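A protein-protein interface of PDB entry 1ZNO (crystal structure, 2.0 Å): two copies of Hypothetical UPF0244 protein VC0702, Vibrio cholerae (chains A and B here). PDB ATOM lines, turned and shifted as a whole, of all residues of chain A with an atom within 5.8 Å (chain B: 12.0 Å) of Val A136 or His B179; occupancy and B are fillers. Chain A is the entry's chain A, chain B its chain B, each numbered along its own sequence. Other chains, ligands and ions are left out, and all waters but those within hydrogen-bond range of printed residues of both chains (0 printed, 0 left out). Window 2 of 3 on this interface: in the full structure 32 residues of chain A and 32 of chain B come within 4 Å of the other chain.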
ATOM      1  N   PRO A 116      14.162  23.501   4.275  1.00  0.00           N
ATOM      2  CA  PRO A 116      13.381  22.971   5.397  1.00  0.00           C
ATOM      3  C   PRO A 116      13.373  21.441   5.338  1.00  0.00           C
ATOM      4  O   PRO A 116      13.270  20.858   4.258  1.00  0.00           O
ATOM      5  CB  PRO A 116      11.989  23.557   5.159  1.00  0.00           C
ATOM      6  CG  PRO A 116      12.268  24.826   4.390  1.00  0.00           C
ATOM      7  CD  PRO A 116      13.342  24.391   3.432  1.00  0.00           C
ATOM      8  N   PRO A 117      13.473  20.773   6.496  1.00  0.00           N
ATOM      9  CA  PRO A 117      13.474  19.308   6.529  1.00  0.00           C
ATOM     10  C   PRO A 117      12.298  18.703   5.768  1.00  0.00           C
ATOM     11  O   PRO A 117      12.431  17.664   5.121  1.00  0.00           O
ATOM     12  CB  PRO A 117      13.422  18.999   8.025  1.00  0.00           C
ATOM     13  CG  PRO A 117      12.667  20.166   8.577  1.00  0.00           C
ATOM     14  CD  PRO A 117      13.323  21.318   7.855  1.00  0.00           C
ATOM     15  N   LEU A 118      11.149  19.368   5.843  1.00  0.00           N
ATOM     16  CA  LEU A 118       9.950  18.901   5.163  1.00  0.00           C
ATOM     17  C   LEU A 118      10.201  18.876   3.659  1.00  0.00           C
ATOM     18  O   LEU A 118       9.610  18.077   2.935  1.00  0.00           O
ATOM     19  CB  LEU A 118       8.769  19.826   5.489  1.00  0.00           C
ATOM     20  CG  LEU A 118       7.335  19.373   5.168  1.00  0.00           C
ATOM     21  CD1 LEU A 118       7.070  19.454   3.676  1.00  0.00           C
ATOM     22  CD2 LEU A 118       7.122  17.954   5.688  1.00  0.00           C
ATOM     23  N   VAL A 132       8.721  20.872  -5.103  1.00  0.00           N
ATOM     24  CA  VAL A 132       8.008  20.620  -3.860  1.00  0.00           C
ATOM     25  C   VAL A 132       7.870  21.990  -3.222  1.00  0.00           C
ATOM     26  O   VAL A 132       6.962  22.251  -2.431  1.00  0.00           O
ATOM     27  CB  VAL A 132       8.825  19.718  -2.915  1.00  0.00           C
ATOM     28  CG1 VAL A 132       8.055  19.480  -1.632  1.00  0.00           C
ATOM     29  CG2 VAL A 132       9.147  18.401  -3.598  1.00  0.00           C
ATOM     30  N   MET A 133       8.798  22.862  -3.596  1.00  0.00           N
ATOM     31  CA  MET A 133       8.846  24.230  -3.105  1.00  0.00           C
ATOM     32  C   MET A 133       7.571  24.960  -3.517  1.00  0.00           C
ATOM     33  O   MET A 133       7.160  25.926  -2.875  1.00  0.00           O
ATOM     34  CB  MET A 133      10.066  24.939  -3.697  1.00  0.00           C
ATOM     35  CG  MET A 133      10.772  25.880  -2.741  1.00  0.00           C
ATOM     36  SD  MET A 133      11.478  24.956  -1.197  1.00  0.00           S
ATOM     37  CE  MET A 133      10.243  25.623   0.133  1.00  0.00           C
ATOM     38  N   ASP A 134       6.950  24.486  -4.594  1.00  0.00           N
ATOM     39  CA  ASP A 134       5.722  25.084  -5.103  1.00  0.00           C
ATOM     40  C   ASP A 134       4.538  24.835  -4.173  1.00  0.00           C
ATOM     41  O   ASP A 134       3.386  25.013  -4.563  1.00  0.00           O
ATOM     42  CB  ASP A 134       5.405  24.532  -6.495  1.00  0.00           C
ATOM     43  CG  ASP A 134       6.388  25.004  -7.548  1.00  0.00           C
ATOM     44  OD1 ASP A 134       6.419  26.223  -7.825  1.00  0.00           O
ATOM     45  OD2 ASP A 134       7.129  24.159  -8.098  1.00  0.00           O
ATOM     46  N   GLU A 135       4.828  24.421  -2.944  1.00  0.00           N
ATOM     47  CA  GLU A 135       3.783  24.161  -1.964  1.00  0.00           C
ATOM     48  C   GLU A 135       3.814  25.197  -0.847  1.00  0.00           C
ATOM     49  O   GLU A 135       3.260  26.289  -0.982  1.00  0.00           O
ATOM     50  CB  GLU A 135       3.947  22.764  -1.369  1.00  0.00           C
ATOM     51  CG  GLU A 135       3.875  21.642  -2.383  1.00  0.00           C
ATOM     52  CD  GLU A 135       3.865  20.275  -1.729  1.00  0.00           C
ATOM     53  OE1 GLU A 135       2.907  19.983  -0.980  1.00  0.00           O
ATOM     54  OE2 GLU A 135       4.815  19.495  -1.960  1.00  0.00           O
ATOM     55  N   VAL A 136       4.471  24.847   0.255  1.00  0.00           N
ATOM     56  CA  VAL A 136       4.578  25.737   1.406  1.00  0.00           C
ATOM     57  C   VAL A 136       6.008  26.235   1.587  1.00  0.00           C
ATOM     58  O   VAL A 136       6.525  26.988   0.761  1.00  0.00           O
ATOM     59  CB  VAL A 136       4.131  25.021   2.701  1.00  0.00           C
ATOM     60  CG1 VAL A 136       5.054  23.849   2.996  1.00  0.00           C
ATOM     61  CG2 VAL A 136       4.118  26.003   3.861  1.00  0.00           C
ATOM     62  N   GLU A 140       0.777  26.706  -6.805  1.00  0.00           N
ATOM     63  CA  GLU A 140       1.240  27.836  -6.010  1.00  0.00           C
ATOM     64  C   GLU A 140       2.480  28.451  -6.645  1.00  0.00           C
ATOM     65  O   GLU A 140       3.483  27.769  -6.873  1.00  0.00           O
ATOM     66  CB  GLU A 140       1.547  27.376  -4.579  1.00  0.00           C
ATOM     67  CG  GLU A 140       1.914  28.489  -3.600  1.00  0.00           C
ATOM     68  CD  GLU A 140       3.410  28.713  -3.488  1.00  0.00           C
ATOM     69  OE1 GLU A 140       3.842  29.358  -2.506  1.00  0.00           O
ATOM     70  OE2 GLU A 140       4.156  28.249  -4.377  1.00  0.00           O
ATOM     71  N   LYS A 143       6.503  31.485  -5.564  1.00  0.00           N
ATOM     72  CA  LYS A 143       7.884  31.174  -5.910  1.00  0.00           C
ATOM     73  C   LYS A 143       8.528  32.271  -6.748  1.00  0.00           C
ATOM     74  O   LYS A 143       9.719  32.539  -6.595  1.00  0.00           O
ATOM     75  CB  LYS A 143       7.961  29.838  -6.658  1.00  0.00           C
ATOM     76  CG  LYS A 143       7.461  28.626  -5.869  1.00  0.00           C
ATOM     77  CD  LYS A 143       8.550  27.926  -5.045  1.00  0.00           C
ATOM     78  CE  LYS A 143       9.106  28.788  -3.918  1.00  0.00           C
ATOM     79  NZ  LYS A 143      10.022  29.854  -4.398  1.00  0.00           N
ATOM     80  N   LEU A 152      12.224  32.665   1.819  1.00  0.00           N
ATOM     81  CA  LEU A 152      12.876  32.317   3.083  1.00  0.00           C
ATOM     82  C   LEU A 152      13.598  33.463   3.790  1.00  0.00           C
ATOM     83  O   LEU A 152      13.765  33.421   5.004  1.00  0.00           O
ATOM     84  CB  LEU A 152      13.848  31.149   2.862  1.00  0.00           C
ATOM     85  CG  LEU A 152      13.212  29.813   2.453  1.00  0.00           C
ATOM     86  CD1 LEU A 152      14.296  28.812   2.048  1.00  0.00           C
ATOM     87  CD2 LEU A 152      12.400  29.269   3.620  1.00  0.00           C
ATOM     88  N   GLN B 104      18.640  26.208  18.397  1.00  0.00           N
ATOM     89  CA  GLN B 104      18.836  25.956  16.978  1.00  0.00           C
ATOM     90  C   GLN B 104      20.119  26.513  16.385  1.00  0.00           C
ATOM     91  O   GLN B 104      20.812  27.320  17.008  1.00  0.00           O
ATOM     92  CB  GLN B 104      17.615  26.448  16.188  1.00  0.00           C
ATOM     93  CG  GLN B 104      17.163  27.852  16.526  1.00  0.00           C
ATOM     94  CD  GLN B 104      15.711  28.107  16.150  1.00  0.00           C
ATOM     95  OE1 GLN B 104      15.252  27.695  15.083  1.00  0.00           O
ATOM     96  NE2 GLN B 104      14.985  28.800  17.024  1.00  0.00           N
ATOM     97  N   ARG B 105      20.438  26.064  15.174  1.00  0.00           N
ATOM     98  CA  ARG B 105      21.652  26.503  14.499  1.00  0.00           C
ATOM     99  C   ARG B 105      21.402  26.881  13.054  1.00  0.00           C
ATOM    100  O   ARG B 105      20.652  26.216  12.359  1.00  0.00           O
ATOM    101  CB  ARG B 105      22.701  25.394  14.522  1.00  0.00           C
ATOM    102  CG  ARG B 105      23.943  25.742  13.715  1.00  0.00           C
ATOM    103  CD  ARG B 105      24.929  24.594  13.694  1.00  0.00           C
ATOM    104  NE  ARG B 105      25.397  24.233  15.026  1.00  0.00           N
ATOM    105  CZ  ARG B 105      25.840  23.022  15.346  1.00  0.00           C
ATOM    106  NH1 ARG B 105      25.869  22.064  14.427  1.00  0.00           N
ATOM    107  NH2 ARG B 105      26.254  22.768  16.579  1.00  0.00           N
ATOM    108  N   GLY B 106      22.041  27.946  12.605  1.00  0.00           N
ATOM    109  CA  GLY B 106      21.883  28.340  11.227  1.00  0.00           C
ATOM    110  C   GLY B 106      23.261  28.370  10.614  1.00  0.00           C
ATOM    111  O   GLY B 106      24.251  28.591  11.316  1.00  0.00           O
ATOM    112  N   LEU B 169      21.502  34.357   4.860  1.00  0.00           N
ATOM    113  CA  LEU B 169      21.136  32.972   4.587  1.00  0.00           C
ATOM    114  C   LEU B 169      21.243  32.130   5.862  1.00  0.00           C
ATOM    115  O   LEU B 169      20.381  31.299   6.135  1.00  0.00           O
ATOM    116  CB  LEU B 169      22.027  32.385   3.476  1.00  0.00           C
ATOM    117  CG  LEU B 169      21.815  33.104   2.141  1.00  0.00           C
ATOM    118  CD1 LEU B 169      22.791  32.628   1.059  1.00  0.00           C
ATOM    119  CD2 LEU B 169      20.373  32.861   1.711  1.00  0.00           C
ATOM    120  N   LEU B 171      20.576  32.924   8.710  1.00  0.00           N
ATOM    121  CA  LEU B 171      19.492  33.247   9.635  1.00  0.00           C
ATOM    122  C   LEU B 171      18.147  32.627   9.260  1.00  0.00           C
ATOM    123  O   LEU B 171      17.190  32.728  10.022  1.00  0.00           O
ATOM    124  CB  LEU B 171      19.317  34.764   9.742  1.00  0.00           C
ATOM    125  CG  LEU B 171      20.410  35.591  10.411  1.00  0.00           C
ATOM    126  CD1 LEU B 171      20.069  37.076  10.283  1.00  0.00           C
ATOM    127  CD2 LEU B 171      20.544  35.209  11.891  1.00  0.00           C
ATOM    128  N   ILE B 172      18.070  32.000   8.089  1.00  0.00           N
ATOM    129  CA  ILE B 172      16.822  31.387   7.638  1.00  0.00           C
ATOM    130  C   ILE B 172      16.093  30.576   8.719  1.00  0.00           C
ATOM    131  O   ILE B 172      14.912  30.801   8.975  1.00  0.00           O
ATOM    132  CB  ILE B 172      17.048  30.498   6.390  1.00  0.00           C
ATOM    133  CG1 ILE B 172      17.063  31.367   5.133  1.00  0.00           C
ATOM    134  CG2 ILE B 172      15.929  29.466   6.259  1.00  0.00           C
ATOM    135  CD1 ILE B 172      18.001  32.539   5.204  1.00  0.00           C
ATOM    136  N   PRO B 173      16.786  29.631   9.367  1.00  0.00           N
ATOM    137  CA  PRO B 173      16.141  28.825  10.412  1.00  0.00           C
ATOM    138  C   PRO B 173      15.429  29.687  11.460  1.00  0.00           C
ATOM    139  O   PRO B 173      14.319  29.368  11.875  1.00  0.00           O
ATOM    140  CB  PRO B 173      17.309  28.036  11.002  1.00  0.00           C
ATOM    141  CG  PRO B 173      18.210  27.844   9.816  1.00  0.00           C
ATOM    142  CD  PRO B 173      18.192  29.226   9.191  1.00  0.00           C
ATOM    143  N   PHE B 174      16.065  30.782  11.865  1.00  0.00           N
ATOM    144  CA  PHE B 174      15.501  31.684  12.870  1.00  0.00           C
ATOM    145  C   PHE B 174      14.396  32.573  12.319  1.00  0.00           C
ATOM    146  O   PHE B 174      13.573  33.093  13.074  1.00  0.00           O
ATOM    147  CB  PHE B 174      16.610  32.553  13.449  1.00  0.00           C
ATOM    148  CG  PHE B 174      17.798  31.766  13.901  1.00  0.00           C
ATOM    149  CD1 PHE B 174      17.777  31.082  15.112  1.00  0.00           C
ATOM    150  CD2 PHE B 174      18.921  31.663  13.086  1.00  0.00           C
ATOM    151  CE1 PHE B 174      18.862  30.301  15.503  1.00  0.00           C
ATOM    152  CE2 PHE B 174      20.011  30.887  13.463  1.00  0.00           C
ATOM    153  CZ  PHE B 174      19.982  30.204  14.675  1.00  0.00           C
ATOM    154  N   ILE B 175      14.387  32.756  11.004  1.00  0.00           N
ATOM    155  CA  ILE B 175      13.374  33.575  10.351  1.00  0.00           C
ATOM    156  C   ILE B 175      12.094  32.771  10.114  1.00  0.00           C
ATOM    157  O   ILE B 175      10.997  33.322  10.136  1.00  0.00           O
ATOM    158  CB  ILE B 175      13.872  34.089   8.978  1.00  0.00           C
ATOM    159  CG1 ILE B 175      15.076  35.011   9.151  1.00  0.00           C
ATOM    160  CG2 ILE B 175      12.759  34.836   8.267  1.00  0.00           C
ATOM    161  CD1 ILE B 175      15.653  35.494   7.823  1.00  0.00           C
ATOM    162  N   ASN B 176      12.241  31.468   9.895  1.00  0.00           N
ATOM    163  CA  ASN B 176      11.101  30.598   9.619  1.00  0.00           C
ATOM    164  C   ASN B 176      10.998  29.419  10.591  1.00  0.00           C
ATOM    165  O   ASN B 176      11.081  28.260  10.184  1.00  0.00           O
ATOM    166  CB  ASN B 176      11.216  30.074   8.188  1.00  0.00           C
ATOM    167  CG  ASN B 176      11.425  31.186   7.181  1.00  0.00           C
ATOM    168  OD1 ASN B 176      10.554  32.027   6.980  1.00  0.00           O
ATOM    169  ND2 ASN B 176      12.587  31.200   6.547  1.00  0.00           N
ATOM    170  N   PRO B 177      10.788  29.701  11.886  1.00  0.00           N
ATOM    171  CA  PRO B 177      10.678  28.657  12.914  1.00  0.00           C
ATOM    172  C   PRO B 177       9.678  27.552  12.591  1.00  0.00           C
ATOM    173  O   PRO B 177       9.870  26.398  12.975  1.00  0.00           O
ATOM    174  CB  PRO B 177      10.269  29.437  14.160  1.00  0.00           C
ATOM    175  CG  PRO B 177      10.870  30.781  13.930  1.00  0.00           C
ATOM    176  CD  PRO B 177      10.553  31.031  12.473  1.00  0.00           C
ATOM    177  N   GLU B 178       8.607  27.911  11.894  1.00  0.00           N
ATOM    178  CA  GLU B 178       7.577  26.940  11.541  1.00  0.00           C
ATOM    179  C   GLU B 178       8.081  25.892  10.550  1.00  0.00           C
ATOM    180  O   GLU B 178       7.430  24.869  10.337  1.00  0.00           O
ATOM    181  CB  GLU B 178       6.354  27.643  10.937  1.00  0.00           C
ATOM    182  CG  GLU B 178       6.240  29.136  11.238  1.00  0.00           C
ATOM    183  CD  GLU B 178       7.271  29.975  10.488  1.00  0.00           C
ATOM    184  OE1 GLU B 178       7.448  29.755   9.271  1.00  0.00           O
ATOM    185  OE2 GLU B 178       7.889  30.864  11.112  1.00  0.00           O
ATOM    186  N   HIS B 179       9.244  26.134   9.955  1.00  0.00           N
ATOM    187  CA  HIS B 179       9.780  25.198   8.972  1.00  0.00           C
ATOM    188  C   HIS B 179      11.099  24.558   9.356  1.00  0.00           C
ATOM    189  O   HIS B 179      11.552  23.628   8.690  1.00  0.00           O
ATOM    190  CB  HIS B 179       9.937  25.911   7.633  1.00  0.00           C
ATOM    191  CG  HIS B 179       8.657  26.469   7.102  1.00  0.00           C
ATOM    192  ND1 HIS B 179       7.707  25.687   6.481  1.00  0.00           N
ATOM    193  CD2 HIS B 179       8.150  27.724   7.135  1.00  0.00           C
ATOM    194  CE1 HIS B 179       6.669  26.437   6.151  1.00  0.00           C
ATOM    195  NE2 HIS B 179       6.914  27.676   6.538  1.00  0.00           N
ATOM    196  N   TYR B 180      11.711  25.057  10.426  1.00  0.00           N
ATOM    197  CA  TYR B 180      12.990  24.539  10.893  1.00  0.00           C
ATOM    198  C   TYR B 180      12.964  24.207  12.384  1.00  0.00           C
ATOM    199  O   TYR B 180      13.377  25.013  13.207  1.00  0.00           O
ATOM    200  CB  TYR B 180      14.102  25.560  10.632  1.00  0.00           C
ATOM    201  CG  TYR B 180      14.317  25.878   9.171  1.00  0.00           C
ATOM    202  CD1 TYR B 180      13.464  26.757   8.487  1.00  0.00           C
ATOM    203  CD2 TYR B 180      15.349  25.264   8.458  1.00  0.00           C
ATOM    204  CE1 TYR B 180      13.635  27.007   7.122  1.00  0.00           C
ATOM    205  CE2 TYR B 180      15.530  25.504   7.105  1.00  0.00           C
ATOM    206  CZ  TYR B 180      14.668  26.372   6.439  1.00  0.00           C
ATOM    207  OH  TYR B 180      14.832  26.566   5.089  1.00  0.00           O
ATOM    208  N   PRO B 181      12.483  23.008  12.745  1.00  0.00           N
ATOM    209  CA  PRO B 181      12.407  22.577  14.145  1.00  0.00           C
ATOM    210  C   PRO B 181      13.761  22.163  14.729  1.00  0.00           C
ATOM    211  O   PRO B 181      14.706  21.864  13.991  1.00  0.00           O
ATOM    212  CB  PRO B 181      11.413  21.424  14.088  1.00  0.00           C
ATOM    213  CG  PRO B 181      11.720  20.804  12.765  1.00  0.00           C
ATOM    214  CD  PRO B 181      11.860  22.011  11.855  1.00  0.00           C
ATOM    215  N   SER B 182      13.840  22.140  16.059  1.00  0.00           N
ATOM    216  CA  SER B 182      15.068  21.777  16.766  1.00  0.00           C
ATOM    217  C   SER B 182      16.249  22.573  16.221  1.00  0.00           C
ATOM    218  O   SER B 182      17.238  21.946  15.776  1.00  0.00           O
ATOM    219  CB  SER B 182      15.348  20.280  16.625  1.00  0.00           C
ATOM    220  OG  SER B 182      14.350  19.508  17.270  1.00  0.00           O
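The backbone carbonyl oxygen (O) of Leu A152 lies within hydrogen-bond range of the side-chain amide nitrogen (ND2) of Asn B176.
The backbone nitrogen of Pro A116 lies close to the side-chain hydroxyl of Tyr B180 (3.2 Å).
O of Ile B172 sits at hydrogen-bond distance from ND2 of Asn B176, 3.4 Å away.
NE2 of His B179 lies close to OE1 of Glu B178, at 3.5 Å.
Among the printed residues, pairs that only touch across the chains: Pro A117 with His B179 (3.0 Å), Val A136 with His B179 (3.5 Å), Pro A116 with His B179 (3.6 Å), Leu A152 with Ile B175 (3.7 Å), Leu A152 with Tyr B180 (3.8 Å), Pro A117 with Pro B181 (3.8 Å) and Leu A152 with Ile B172 (3.9 Å).
Pro A116 touches two residues of chain B.
No residue of chain B comes within 4 Å of Leu A118.
No residue of chain B comes within 4 Å of Met A133.
Glu A135 touches none of the printed residues of chain B.
Val A136 touches just one residue of chain B: His B179 (3.5 Å).
Printed residues of chain B within 4 Å of Leu A152: Ile B172, Ile B175, Asn B176 and Tyr B180.
Printed residues of chain A within 4 Å of Ile B172: Leu A152 (3.9 Å).
Printed residues of chain A within 4 Å of Asn B176: Leu A152.
Of chain A, only Pro A116, Pro A117 and Val A136 come within 4 Å of His B179.
Printed residues of chain A within 4 Å of Tyr B180: Pro A116 and Leu A152.
Of the printed residues of chain A, Pro B181 touches Pro A117 (3.8 Å).
The nearest residue of chain B that does not touch Val A136 is Glu B178 (7.4 Å).
The nearest residue of chain A that does not touch His B179 is Leu A118 (5.1 Å).
Of the 16 printed residues of chain B, 6 touch a printed residue of chain A.
Printed residues of chain B that touch a printed residue of chain A: Ile B172, Ile B175, Asn B176, His B179, Tyr B180 and Pro B181.
Of the 11 printed residues of chain A, 4 touch a printed residue of chain B.
Printed residues of chain A that touch a printed residue of chain B: Pro A116, Pro A117, Val A136 and Leu A152.
Hydrophobic or aromatic side chains of chain A that line the printed part of chain B: Pro A116, Pro A117, Val A136 and Leu A152.
Among the printed residues, 9 pairs touch across the chains.
Among the printed residues, no Asp or Glu carboxylate lies within 4 Å of a Lys or Arg side-chain nitrogen of the other chain.
No position is printed for both chains.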
